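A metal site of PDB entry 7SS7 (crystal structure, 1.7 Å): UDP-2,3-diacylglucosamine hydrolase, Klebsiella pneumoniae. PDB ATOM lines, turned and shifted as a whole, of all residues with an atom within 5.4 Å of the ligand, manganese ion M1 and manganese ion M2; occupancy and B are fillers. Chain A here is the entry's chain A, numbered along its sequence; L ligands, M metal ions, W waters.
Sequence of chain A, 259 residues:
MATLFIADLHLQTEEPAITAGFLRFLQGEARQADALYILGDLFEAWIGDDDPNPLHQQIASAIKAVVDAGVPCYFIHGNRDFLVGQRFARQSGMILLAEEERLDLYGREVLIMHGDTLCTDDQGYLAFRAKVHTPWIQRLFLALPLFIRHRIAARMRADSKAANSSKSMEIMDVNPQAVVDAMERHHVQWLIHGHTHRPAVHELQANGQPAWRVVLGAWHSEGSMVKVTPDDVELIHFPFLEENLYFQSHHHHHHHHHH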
ATOM      1  N   ASP A   8      -9.914 -27.210   2.077  1.00  0.00           N
ATOM      2  CA  ASP A   8     -10.269 -26.873   3.446  1.00  0.00           C
ATOM      3  C   ASP A   8      -9.792 -25.472   3.846  1.00  0.00           C
ATOM      4  O   ASP A   8      -9.310 -25.236   4.960  1.00  0.00           O
ATOM      5  CB  ASP A   8      -9.721 -27.947   4.401  1.00  0.00           C
ATOM      6  CG  ASP A   8     -10.369 -29.292   4.132  1.00  0.00           C
ATOM      7  OD1 ASP A   8     -11.600 -29.378   4.287  1.00  0.00           O
ATOM      8  OD2 ASP A   8      -9.675 -30.247   3.749  1.00  0.00           O
ATOM      9  N   HIS A  10     -12.177 -22.978   3.824  1.00  0.00           N
ATOM     10  CA  HIS A  10     -13.397 -22.525   4.527  1.00  0.00           C
ATOM     11  C   HIS A  10     -13.509 -21.008   4.500  1.00  0.00           C
ATOM     12  O   HIS A  10     -13.776 -20.357   5.520  1.00  0.00           O
ATOM     13  CB  HIS A  10     -13.444 -23.050   5.969  1.00  0.00           C
ATOM     14  CG  HIS A  10     -13.076 -24.491   6.095  1.00  0.00           C
ATOM     15  ND1 HIS A  10     -11.883 -24.908   6.641  1.00  0.00           N
ATOM     16  CD2 HIS A  10     -13.736 -25.627   5.728  1.00  0.00           C
ATOM     17  CE1 HIS A  10     -11.819 -26.223   6.605  1.00  0.00           C
ATOM     18  NE2 HIS A  10     -12.927 -26.683   6.049  1.00  0.00           N
ATOM     19  N   ASP A  41     -14.207 -27.800   0.012  1.00  0.00           N
ATOM     20  CA  ASP A  41     -14.261 -26.895   1.159  1.00  0.00           C
ATOM     21  C   ASP A  41     -13.430 -25.642   0.911  1.00  0.00           C
ATOM     22  O   ASP A  41     -12.732 -25.130   1.798  1.00  0.00           O
ATOM     23  CB  ASP A  41     -13.854 -27.608   2.458  1.00  0.00           C
ATOM     24  CG  ASP A  41     -14.940 -28.530   2.973  1.00  0.00           C
ATOM     25  OD1 ASP A  41     -15.993 -28.640   2.303  1.00  0.00           O
ATOM     26  OD2 ASP A  41     -14.739 -29.152   4.023  1.00  0.00           O
ATOM     27  N   GLU A  44     -16.700 -21.851   3.284  1.00  0.00           N
ATOM     28  CA  GLU A  44     -17.334 -22.404   4.492  1.00  0.00           C
ATOM     29  C   GLU A  44     -18.798 -22.740   4.265  1.00  0.00           C
ATOM     30  O   GLU A  44     -19.358 -23.582   4.983  1.00  0.00           O
ATOM     31  CB  GLU A  44     -17.186 -21.417   5.663  1.00  0.00           C
ATOM     32  CG  GLU A  44     -17.984 -21.783   6.932  1.00  0.00           C
ATOM     33  CD  GLU A  44     -17.570 -23.076   7.615  1.00  0.00           C
ATOM     34  OE1 GLU A  44     -18.209 -23.436   8.623  1.00  0.00           O
ATOM     35  OE2 GLU A  44     -16.603 -23.736   7.184  1.00  0.00           O
ATOM     36  N   ALA A  45     -19.440 -22.113   3.273  1.00  0.00           N
ATOM     37  CA  ALA A  45     -20.841 -22.385   2.991  1.00  0.00           C
ATOM     38  C   ALA A  45     -21.101 -22.043   1.530  1.00  0.00           C
ATOM     39  O   ALA A  45     -20.363 -21.273   0.907  1.00  0.00           O
ATOM     40  CB  ALA A  45     -21.758 -21.560   3.905  1.00  0.00           C
ATOM     41  N   TRP A  46     -22.142 -22.658   0.958  1.00  0.00           N
ATOM     42  CA  TRP A  46     -22.588 -22.282  -0.387  1.00  0.00           C
ATOM     43  C   TRP A  46     -24.061 -22.603  -0.496  1.00  0.00           C
ATOM     44  O   TRP A  46     -24.455 -23.744  -0.204  1.00  0.00           O
ATOM     45  CB  TRP A  46     -21.813 -23.036  -1.480  1.00  0.00           C
ATOM     46  CG  TRP A  46     -21.852 -22.353  -2.831  1.00  0.00           C
ATOM     47  CD1 TRP A  46     -22.713 -22.599  -3.864  1.00  0.00           C
ATOM     48  CD2 TRP A  46     -20.955 -21.341  -3.282  1.00  0.00           C
ATOM     49  NE1 TRP A  46     -22.405 -21.775  -4.938  1.00  0.00           N
ATOM     50  CE2 TRP A  46     -21.323 -20.995  -4.598  1.00  0.00           C
ATOM     51  CE3 TRP A  46     -19.878 -20.674  -2.687  1.00  0.00           C
ATOM     52  CZ2 TRP A  46     -20.641 -20.032  -5.345  1.00  0.00           C
ATOM     53  CZ3 TRP A  46     -19.188 -19.710  -3.439  1.00  0.00           C
ATOM     54  CH2 TRP A  46     -19.578 -19.396  -4.743  1.00  0.00           C
ATOM     55  N   ILE A  47     -24.861 -21.635  -0.921  1.00  0.00           N
ATOM     56  CA  ILE A  47     -26.294 -21.867  -1.073  1.00  0.00           C
ATOM     57  C   ILE A  47     -26.753 -21.706  -2.522  1.00  0.00           C
ATOM     58  O   ILE A  47     -27.957 -21.687  -2.779  1.00  0.00           O
ATOM     59  CB  ILE A  47     -27.129 -20.970  -0.128  1.00  0.00           C
ATOM     60  CG1 ILE A  47     -26.858 -19.481  -0.415  1.00  0.00           C
ATOM     61  CG2 ILE A  47     -26.836 -21.323   1.348  1.00  0.00           C
ATOM     62  CD1 ILE A  47     -27.763 -18.529   0.329  1.00  0.00           C
ATOM     63  N   GLY A  78     -16.445 -30.073  -1.773  1.00  0.00           N
ATOM     64  CA  GLY A  78     -16.401 -30.522  -0.393  1.00  0.00           C
ATOM     65  C   GLY A  78     -17.810 -30.683   0.182  1.00  0.00           C
ATOM     66  O   GLY A  78     -18.810 -30.450  -0.481  1.00  0.00           O
ATOM     67  N   ASN A  79     -17.867 -31.098   1.448  1.00  0.00           N
ATOM     68  CA  ASN A  79     -19.169 -31.175   2.105  1.00  0.00           C
ATOM     69  C   ASN A  79     -19.722 -29.782   2.460  1.00  0.00           C
ATOM     70  O   ASN A  79     -20.932 -29.646   2.650  1.00  0.00           O
ATOM     71  CB  ASN A  79     -19.075 -32.035   3.365  1.00  0.00           C
ATOM     72  CG  ASN A  79     -18.040 -31.534   4.321  1.00  0.00           C
ATOM     73  OD1 ASN A  79     -16.851 -31.606   4.048  1.00  0.00           O
ATOM     74  ND2 ASN A  79     -18.483 -31.005   5.463  1.00  0.00           N
ATOM     75  N   ARG A  80     -18.870 -28.763   2.561  1.00  0.00           N
ATOM     76  CA  ARG A  80     -19.405 -27.431   2.841  1.00  0.00           C
ATOM     77  C   ARG A  80     -19.932 -26.761   1.581  1.00  0.00           C
ATOM     78  O   ARG A  80     -20.929 -26.014   1.638  1.00  0.00           O
ATOM     79  CB  ARG A  80     -18.334 -26.518   3.471  1.00  0.00           C
ATOM     80  CG  ARG A  80     -17.697 -27.074   4.741  1.00  0.00           C
ATOM     81  CD  ARG A  80     -18.764 -27.342   5.819  1.00  0.00           C
ATOM     82  NE  ARG A  80     -19.506 -26.125   6.165  1.00  0.00           N
ATOM     83  CZ  ARG A  80     -20.348 -26.055   7.183  1.00  0.00           C
ATOM     84  NH1 ARG A  80     -20.566 -27.095   7.978  1.00  0.00           N
ATOM     85  NH2 ARG A  80     -20.974 -24.910   7.417  1.00  0.00           N
ATOM     86  N   PHE A  82     -20.801 -28.141  -1.631  1.00  0.00           N
ATOM     87  CA  PHE A  82     -21.259 -29.056  -2.667  1.00  0.00           C
ATOM     88  C   PHE A  82     -22.208 -28.414  -3.672  1.00  0.00           C
ATOM     89  O   PHE A  82     -22.434 -28.984  -4.748  1.00  0.00           O
ATOM     90  CB  PHE A  82     -21.936 -30.300  -2.036  1.00  0.00           C
ATOM     91  CG  PHE A  82     -23.137 -29.992  -1.156  1.00  0.00           C
ATOM     92  CD1 PHE A  82     -22.981 -29.736   0.219  1.00  0.00           C
ATOM     93  CD2 PHE A  82     -24.420 -30.006  -1.684  1.00  0.00           C
ATOM     94  CE1 PHE A  82     -24.097 -29.473   1.029  1.00  0.00           C
ATOM     95  CE2 PHE A  82     -25.534 -29.741  -0.892  1.00  0.00           C
ATOM     96  CZ  PHE A  82     -25.373 -29.476   0.473  1.00  0.00           C
ATOM     97  N   LEU A  83     -22.772 -27.238  -3.374  1.00  0.00           N
ATOM     98  CA  LEU A  83     -23.665 -26.578  -4.329  1.00  0.00           C
ATOM     99  C   LEU A  83     -22.951 -25.672  -5.319  1.00  0.00           C
ATOM    100  O   LEU A  83     -23.615 -25.032  -6.131  1.00  0.00           O
ATOM    101  CB  LEU A  83     -24.747 -25.778  -3.608  1.00  0.00           C
ATOM    102  CG  LEU A  83     -25.815 -26.604  -2.891  1.00  0.00           C
ATOM    103  CD1 LEU A  83     -26.861 -25.675  -2.249  1.00  0.00           C
ATOM    104  CD2 LEU A  83     -26.502 -27.609  -3.849  1.00  0.00           C
ATOM    105  N   HIS A 114     -12.203 -35.228  -2.119  1.00  0.00           N
ATOM    106  CA  HIS A 114     -12.280 -34.405  -0.914  1.00  0.00           C
ATOM    107  C   HIS A 114     -11.901 -35.215   0.316  1.00  0.00           C
ATOM    108  O   HIS A 114     -11.192 -34.715   1.197  1.00  0.00           O
ATOM    109  CB  HIS A 114     -13.677 -33.785  -0.729  1.00  0.00           C
ATOM    110  CG  HIS A 114     -13.769 -32.937   0.501  1.00  0.00           C
ATOM    111  ND1 HIS A 114     -12.955 -31.844   0.729  1.00  0.00           N
ATOM    112  CD2 HIS A 114     -14.577 -33.028   1.592  1.00  0.00           C
ATOM    113  CE1 HIS A 114     -13.249 -31.305   1.896  1.00  0.00           C
ATOM    114  NE2 HIS A 114     -14.227 -32.000   2.441  1.00  0.00           N
ATOM    115  N   ASP A 116     -14.361 -37.009   2.325  1.00  0.00           N
ATOM    116  CA  ASP A 116     -15.439 -37.348   3.247  1.00  0.00           C
ATOM    117  C   ASP A 116     -16.070 -38.700   2.921  1.00  0.00           C
ATOM    118  O   ASP A 116     -16.586 -39.370   3.830  1.00  0.00           O
ATOM    119  CB  ASP A 116     -16.514 -36.249   3.261  1.00  0.00           C
ATOM    120  CG  ASP A 116     -17.118 -35.995   1.900  1.00  0.00           C
ATOM    121  OD1 ASP A 116     -16.379 -35.796   0.913  1.00  0.00           O
ATOM    122  OD2 ASP A 116     -18.360 -35.984   1.807  1.00  0.00           O
ATOM    123  N   TYR A 125     -23.555 -39.451   8.795  1.00  0.00           N
ATOM    124  CA  TYR A 125     -23.084 -38.454   7.856  1.00  0.00           C
ATOM    125  C   TYR A 125     -23.316 -38.901   6.419  1.00  0.00           C
ATOM    126  O   TYR A 125     -23.788 -38.117   5.590  1.00  0.00           O
ATOM    127  CB  TYR A 125     -21.610 -38.151   8.068  1.00  0.00           C
ATOM    128  CG  TYR A 125     -21.077 -37.317   6.923  1.00  0.00           C
ATOM    129  CD1 TYR A 125     -21.465 -35.999   6.780  1.00  0.00           C
ATOM    130  CD2 TYR A 125     -20.259 -37.875   5.942  1.00  0.00           C
ATOM    131  CE1 TYR A 125     -21.020 -35.231   5.728  1.00  0.00           C
ATOM    132  CE2 TYR A 125     -19.814 -37.112   4.865  1.00  0.00           C
ATOM    133  CZ  TYR A 125     -20.197 -35.791   4.775  1.00  0.00           C
ATOM    134  OH  TYR A 125     -19.759 -35.022   3.711  1.00  0.00           O
ATOM    135  N   PHE A 128     -26.900 -38.355   5.336  1.00  0.00           N
ATOM    136  CA  PHE A 128     -27.115 -36.941   5.056  1.00  0.00           C
ATOM    137  C   PHE A 128     -26.471 -36.532   3.726  1.00  0.00           C
ATOM    138  O   PHE A 128     -27.077 -35.806   2.926  1.00  0.00           O
ATOM    139  CB  PHE A 128     -26.546 -36.108   6.207  1.00  0.00           C
ATOM    140  CG  PHE A 128     -26.445 -34.642   5.913  1.00  0.00           C
ATOM    141  CD1 PHE A 128     -27.538 -33.818   6.055  1.00  0.00           C
ATOM    142  CD2 PHE A 128     -25.238 -34.094   5.490  1.00  0.00           C
ATOM    143  CE1 PHE A 128     -27.453 -32.457   5.782  1.00  0.00           C
ATOM    144  CE2 PHE A 128     -25.142 -32.745   5.210  1.00  0.00           C
ATOM    145  CZ  PHE A 128     -26.252 -31.923   5.362  1.00  0.00           C
ATOM    146  N   VAL A 132     -28.384 -34.740   0.371  1.00  0.00           N
ATOM    147  CA  VAL A 132     -28.083 -33.435  -0.235  1.00  0.00           C
ATOM    148  C   VAL A 132     -27.379 -33.562  -1.582  1.00  0.00           C
ATOM    149  O   VAL A 132     -27.260 -32.558  -2.294  1.00  0.00           O
ATOM    150  CB  VAL A 132     -27.276 -32.496   0.689  1.00  0.00           C
ATOM    151  CG1 VAL A 132     -28.056 -32.195   1.978  1.00  0.00           C
ATOM    152  CG2 VAL A 132     -25.872 -33.053   0.998  1.00  0.00           C
ATOM    153  N   ILE A 137     -33.463 -33.086  -4.920  1.00  0.00           N
ATOM    154  CA  ILE A 137     -33.442 -32.317  -3.680  1.00  0.00           C
ATOM    155  C   ILE A 137     -32.650 -31.038  -3.883  1.00  0.00           C
ATOM    156  O   ILE A 137     -33.075 -29.950  -3.461  1.00  0.00           O
ATOM    157  CB  ILE A 137     -32.888 -33.181  -2.529  1.00  0.00           C
ATOM    158  CG1 ILE A 137     -33.854 -34.333  -2.261  1.00  0.00           C
ATOM    159  CG2 ILE A 137     -32.694 -32.325  -1.274  1.00  0.00           C
ATOM    160  CD1 ILE A 137     -33.436 -35.245  -1.103  1.00  0.00           C
ATOM    161  N   GLN A 138     -31.502 -31.110  -4.559  1.00  0.00           N
ATOM    162  CA  GLN A 138     -30.760 -29.892  -4.857  1.00  0.00           C
ATOM    163  C   GLN A 138     -31.587 -28.928  -5.684  1.00  0.00           C
ATOM    164  O   GLN A 138     -31.570 -27.716  -5.446  1.00  0.00           O
ATOM    165  CB  GLN A 138     -29.448 -30.223  -5.581  1.00  0.00           C
ATOM    166  CG  GLN A 138     -28.454 -30.986  -4.732  1.00  0.00           C
ATOM    167  CD  GLN A 138     -27.121 -31.096  -5.420  1.00  0.00           C
ATOM    168  OE1 GLN A 138     -26.968 -30.653  -6.559  1.00  0.00           O
ATOM    169  NE2 GLN A 138     -26.129 -31.671  -4.724  1.00  0.00           N
ATOM    170  N   PHE A 141     -34.141 -27.164  -3.438  1.00  0.00           N
ATOM    171  CA  PHE A 141     -33.503 -26.179  -2.559  1.00  0.00           C
ATOM    172  C   PHE A 141     -33.087 -24.941  -3.340  1.00  0.00           C
ATOM    173  O   PHE A 141     -33.355 -23.808  -2.929  1.00  0.00           O
ATOM    174  CB  PHE A 141     -32.294 -26.804  -1.860  1.00  0.00           C
ATOM    175  CG  PHE A 141     -31.524 -25.818  -1.011  1.00  0.00           C
ATOM    176  CD1 PHE A 141     -31.946 -25.525   0.280  1.00  0.00           C
ATOM    177  CD2 PHE A 141     -30.407 -25.172  -1.527  1.00  0.00           C
ATOM    178  CE1 PHE A 141     -31.234 -24.619   1.053  1.00  0.00           C
ATOM    179  CE2 PHE A 141     -29.700 -24.258  -0.760  1.00  0.00           C
ATOM    180  CZ  PHE A 141     -30.113 -23.984   0.518  1.00  0.00           C
ATOM    181  N   ILE A 152     -32.154 -20.707   6.026  1.00  0.00           N
ATOM    182  CA  ILE A 152     -31.973 -22.131   6.284  1.00  0.00           C
ATOM    183  C   ILE A 152     -30.532 -22.409   6.655  1.00  0.00           C
ATOM    184  O   ILE A 152     -30.241 -23.124   7.623  1.00  0.00           O
ATOM    185  CB  ILE A 152     -32.400 -22.950   5.058  1.00  0.00           C
ATOM    186  CG1 ILE A 152     -33.917 -22.900   4.849  1.00  0.00           C
ATOM    187  CG2 ILE A 152     -31.938 -24.391   5.167  1.00  0.00           C
ATOM    188  CD1 ILE A 152     -34.315 -23.483   3.527  1.00  0.00           C
ATOM    189  N   ALA A 153     -29.593 -21.820   5.911  1.00  0.00           N
ATOM    190  CA  ALA A 153     -28.179 -22.074   6.153  1.00  0.00           C
ATOM    191  C   ALA A 153     -27.740 -21.518   7.500  1.00  0.00           C
ATOM    192  O   ALA A 153     -26.985 -22.173   8.239  1.00  0.00           O
ATOM    193  CB  ALA A 153     -27.341 -21.480   5.022  1.00  0.00           C
ATOM    194  N   MET A 156     -29.086 -23.757  10.224  1.00  0.00           N
ATOM    195  CA  MET A 156     -28.352 -25.025  10.346  1.00  0.00           C
ATOM    196  C   MET A 156     -27.032 -24.834  11.077  1.00  0.00           C
ATOM    197  O   MET A 156     -26.565 -25.747  11.761  1.00  0.00           O
ATOM    198  CB  MET A 156     -28.135 -25.638   8.961  1.00  0.00           C
ATOM    199  CG  MET A 156     -29.359 -26.357   8.395  1.00  0.00           C
ATOM    200  SD  MET A 156     -29.241 -26.861   6.665  1.00  0.00           S
ATOM    201  CE  MET A 156     -28.176 -28.292   6.790  1.00  0.00           C
ATOM    202  N   MET A 172     -14.497 -36.581  12.071  1.00  0.00           N
ATOM    203  CA  MET A 172     -14.335 -37.975  11.691  1.00  0.00           C
ATOM    204  C   MET A 172     -13.041 -38.195  10.909  1.00  0.00           C
ATOM    205  O   MET A 172     -12.532 -37.280  10.252  1.00  0.00           O
ATOM    206  CB  MET A 172     -15.534 -38.409  10.840  1.00  0.00           C
ATOM    207  CG  MET A 172     -15.743 -37.526   9.610  1.00  0.00           C
ATOM    208  SD  MET A 172     -17.459 -37.367   9.061  1.00  0.00           S
ATOM    209  CE  MET A 172     -17.622 -35.586   9.037  1.00  0.00           C
ATOM    210  N   HIS A 195     -10.534 -32.866   3.984  1.00  0.00           N
ATOM    211  CA  HIS A 195     -11.677 -33.167   4.861  1.00  0.00           C
ATOM    212  C   HIS A 195     -11.309 -33.436   6.315  1.00  0.00           C
ATOM    213  O   HIS A 195     -11.973 -32.890   7.214  1.00  0.00           O
ATOM    214  CB  HIS A 195     -12.505 -34.357   4.373  1.00  0.00           C
ATOM    215  CG  HIS A 195     -13.770 -34.528   5.152  1.00  0.00           C
ATOM    216  ND1 HIS A 195     -14.773 -33.583   5.162  1.00  0.00           N
ATOM    217  CD2 HIS A 195     -14.186 -35.520   5.981  1.00  0.00           C
ATOM    218  CE1 HIS A 195     -15.752 -33.988   5.942  1.00  0.00           C
ATOM    219  NE2 HIS A 195     -15.431 -35.167   6.446  1.00  0.00           N
ATOM    220  N   THR A 196     -10.316 -34.282   6.585  1.00  0.00           N
ATOM    221  CA  THR A 196     -10.075 -34.682   7.966  1.00  0.00           C
ATOM    222  C   THR A 196      -9.257 -33.668   8.742  1.00  0.00           C
ATOM    223  O   THR A 196      -9.141 -33.788   9.966  1.00  0.00           O
ATOM    224  CB  THR A 196      -9.377 -36.047   8.007  1.00  0.00           C
ATOM    225  OG1 THR A 196      -8.111 -35.946   7.355  1.00  0.00           O
ATOM    226  CG2 THR A 196     -10.225 -37.086   7.295  1.00  0.00           C
ATOM    227  N   HIS A 197      -8.668 -32.675   8.069  1.00  0.00           N
ATOM    228  CA  HIS A 197      -7.917 -31.607   8.714  1.00  0.00           C
ATOM    229  C   HIS A 197      -6.740 -32.141   9.538  1.00  0.00           C
ATOM    230  O   HIS A 197      -6.393 -31.563  10.565  1.00  0.00           O
ATOM    231  CB  HIS A 197      -8.834 -30.750   9.598  1.00  0.00           C
ATOM    232  CG  HIS A 197      -9.962 -30.083   8.873  1.00  0.00           C
ATOM    233  ND1 HIS A 197     -10.862 -29.247   9.498  1.00  0.00           N
ATOM    234  CD2 HIS A 197     -10.330 -30.117   7.569  1.00  0.00           C
ATOM    235  CE1 HIS A 197     -11.742 -28.801   8.618  1.00  0.00           C
ATOM    236  NE2 HIS A 197     -11.448 -29.324   7.436  1.00  0.00           N
HETATM  237  C1  LIG L   1     -24.501 -26.362   6.231  1.00  0.00           C
HETATM  238  C2  LIG L   1     -23.337 -28.448   6.370  1.00  0.00           C
HETATM  239  C3  LIG L   1     -23.062 -27.069   4.411  1.00  0.00           C
HETATM  240  C4  LIG L   1     -20.445 -32.360   7.838  1.00  0.00           C
HETATM  241  C5  LIG L   1     -18.001 -32.110   8.462  1.00  0.00           C
HETATM  242  C6  LIG L   1     -16.891 -29.858   8.155  1.00  0.00           C
HETATM  243  C7  LIG L   1     -28.823 -28.054   0.646  1.00  0.00           C
HETATM  244  C8  LIG L   1     -28.960 -27.426   1.860  1.00  0.00           C
HETATM  245  C9  LIG L   1     -26.842 -26.202   1.392  1.00  0.00           C
HETATM  246  C10 LIG L   1     -25.570 -26.055   2.211  1.00  0.00           C
HETATM  247  C11 LIG L   1     -26.906 -25.364   4.112  1.00  0.00           C
HETATM  248  C12 LIG L   1     -28.181 -25.534   3.302  1.00  0.00           C
HETATM  249  C13 LIG L   1     -23.924 -26.151   4.986  1.00  0.00           C
HETATM  250  C14 LIG L   1     -24.198 -27.514   6.930  1.00  0.00           C
HETATM  251  C15 LIG L   1     -22.777 -28.224   5.118  1.00  0.00           C
HETATM  252  C16 LIG L   1     -21.822 -30.430   7.063  1.00  0.00           C
HETATM  253  C17 LIG L   1     -19.447 -31.707   8.803  1.00  0.00           C
HETATM  254  C18 LIG L   1     -16.977 -31.118   9.032  1.00  0.00           C
HETATM  255  C19 LIG L   1     -15.594 -29.744   7.349  1.00  0.00           C
HETATM  256  C20 LIG L   1     -30.065 -27.629   2.673  1.00  0.00           C
HETATM  257  C21 LIG L   1     -31.042 -28.491   2.218  1.00  0.00           C
HETATM  258  C22 LIG L   1     -30.927 -29.151   1.014  1.00  0.00           C
HETATM  259  C23 LIG L   1     -29.804 -28.920   0.226  1.00  0.00           C
HETATM  260  C24 LIG L   1     -32.259 -28.711   3.114  1.00  0.00           C
HETATM  261  F1  LIG L   1     -31.821 -29.226   4.282  1.00  0.00           F
HETATM  262  F2  LIG L   1     -33.123 -29.553   2.488  1.00  0.00           F
HETATM  263  F3  LIG L   1     -32.878 -27.529   3.353  1.00  0.00           F
HETATM  264  N1  LIG L   1     -27.935 -26.527   2.290  1.00  0.00           N
HETATM  265  N2  LIG L   1     -25.754 -25.073   3.270  1.00  0.00           N
HETATM  266  N3  LIG L   1     -23.047 -29.638   7.138  1.00  0.00           N
HETATM  267  N4  LIG L   1     -21.671 -31.589   7.906  1.00  0.00           N
HETATM  268  N5  LIG L   1     -14.936 -30.961   6.888  1.00  0.00           N
HETATM  269  O1  LIG L   1     -24.602 -23.589   5.053  1.00  0.00           O
HETATM  270  O2  LIG L   1     -23.341 -24.316   3.126  1.00  0.00           O
HETATM  271  O3  LIG L   1     -20.941 -30.143   6.315  1.00  0.00           O
HETATM  272  O4  LIG L   1     -15.094 -28.673   7.103  1.00  0.00           O
HETATM  273  O5  LIG L   1     -13.732 -30.859   6.140  1.00  0.00           O
HETATM  274  S1  LIG L   1     -24.364 -24.661   4.107  1.00  0.00           S
HETATM  275 CL1  LIG L   1     -29.587 -29.708  -1.333  1.00  0.00          CL
HETATM  276 MN    MN M   1     -13.024 -28.917   5.739  1.00  0.00          MN
HETATM  277 MN    MN M   2     -14.972 -31.395   4.498  1.00  0.00          MN
HETATM  278  O   HOH W   1     -16.180 -26.220   8.144  1.00  0.00           O
HETATM  279  O   HOH W   2     -24.070 -23.049   7.904  1.00  0.00           O
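Of the 27 residues printed, 4 come within 4 Å of manganese ion M1. The nearest printed residue that does not touch manganese ion M1 is His 195 (4.4 Å).
The backbone carbonyl oxygen (O) of His 195 lies close to an oxygen (O5) of the ligand (2.9 Å). The backbone NH (N) of Trp 46 is in hydrogen-bond range of an oxygen (O2) of the ligand (3.0 Å). The guanidinium group (NH1) of Arg 80 lies close to an oxygen (O3) of the ligand, 3.5 Å away.
Manganese ion M2 is bound by OD1 of Asn 79, O5 of the ligand, NE2 of His 114, ND1 of His 195 and OD2 of Asp 41.
Manganese ion M1 is bound by OD1 of Asp 8 (2.1 Å), O5 of the ligand (2.1 Å), NE2 of His 10 (2.3 Å), NE2 of His 197 (2.4 Å), OD2 of Asp 41 (2.4 Å) and O4 of the ligand (2.5 Å). Manganese ion M1 has six donor atoms within binding distance.
Five residues have an atom within 4 Å of manganese ion M2: Asp 8, Asp 41, Asn 79, His 114 and His 195.
The side-chain carboxylate (OD2) of Asp 8 lies within hydrogen-bond range of the backbone NH (N) of His 195 (2.8 Å). The backbone NH (N) of Arg 80 is in hydrogen-bond range of the side-chain carboxylate (OD1) of Asp 41, at 2.9 Å. NH2 of Arg 80 lies within salt-bridge range of OE1 of Glu 44. OD2 of Asp 116 lies within hydrogen-bond range of OH of Tyr 125 (2.6 Å). The side-chain amide nitrogen (NE2) of Gln 138 sits at hydrogen-bond distance from the backbone carbonyl oxygen (O) of Val 132.
Water W2 bridges an oxygen (O1) of the ligand (3.0 Å) and the backbone carbonyl oxygen of Ala 153 (3.1 Å).
Ala 45 touches the ligand (CA to O2, 3.2 Å). CZ of Phe 82 touches C9 of the ligand, 3.7 Å away. Leu 83 touches the ligand (CD1 to C9, 3.7 Å). Tyr 125 touches the ligand (CE1 to C4, 3.6 Å). O of Val 132 touches CL1 of the ligand, 3.8 Å away. CA of Gln 138 touches CL1 of the ligand, at 3.7 Å. Phe 141 touches the ligand (CE1 to C20, 3.6 Å). Ile 152 touches the ligand (CG2 to F3, 3.7 Å). Ala 153 touches the ligand (CB to O1, 3.5 Å). Met 156 touches the ligand (SD to C12, 3.8 Å). Met 172 touches the ligand (CE to C5, 3.5 Å). Within 4 Å of the ligand: Asp 8, His 10, Asp 41, Ala 45, Trp 46, Asn 79, Arg 80, Phe 82, Leu 83, His 114, Tyr 125, Val 132, Gln 138, Phe 141, Ile 152, Ala 153, Met 156, Met 172, His 195 and His 197. The nearest printed residue that does not touch the ligand is Ile 137 (4.1 Å).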
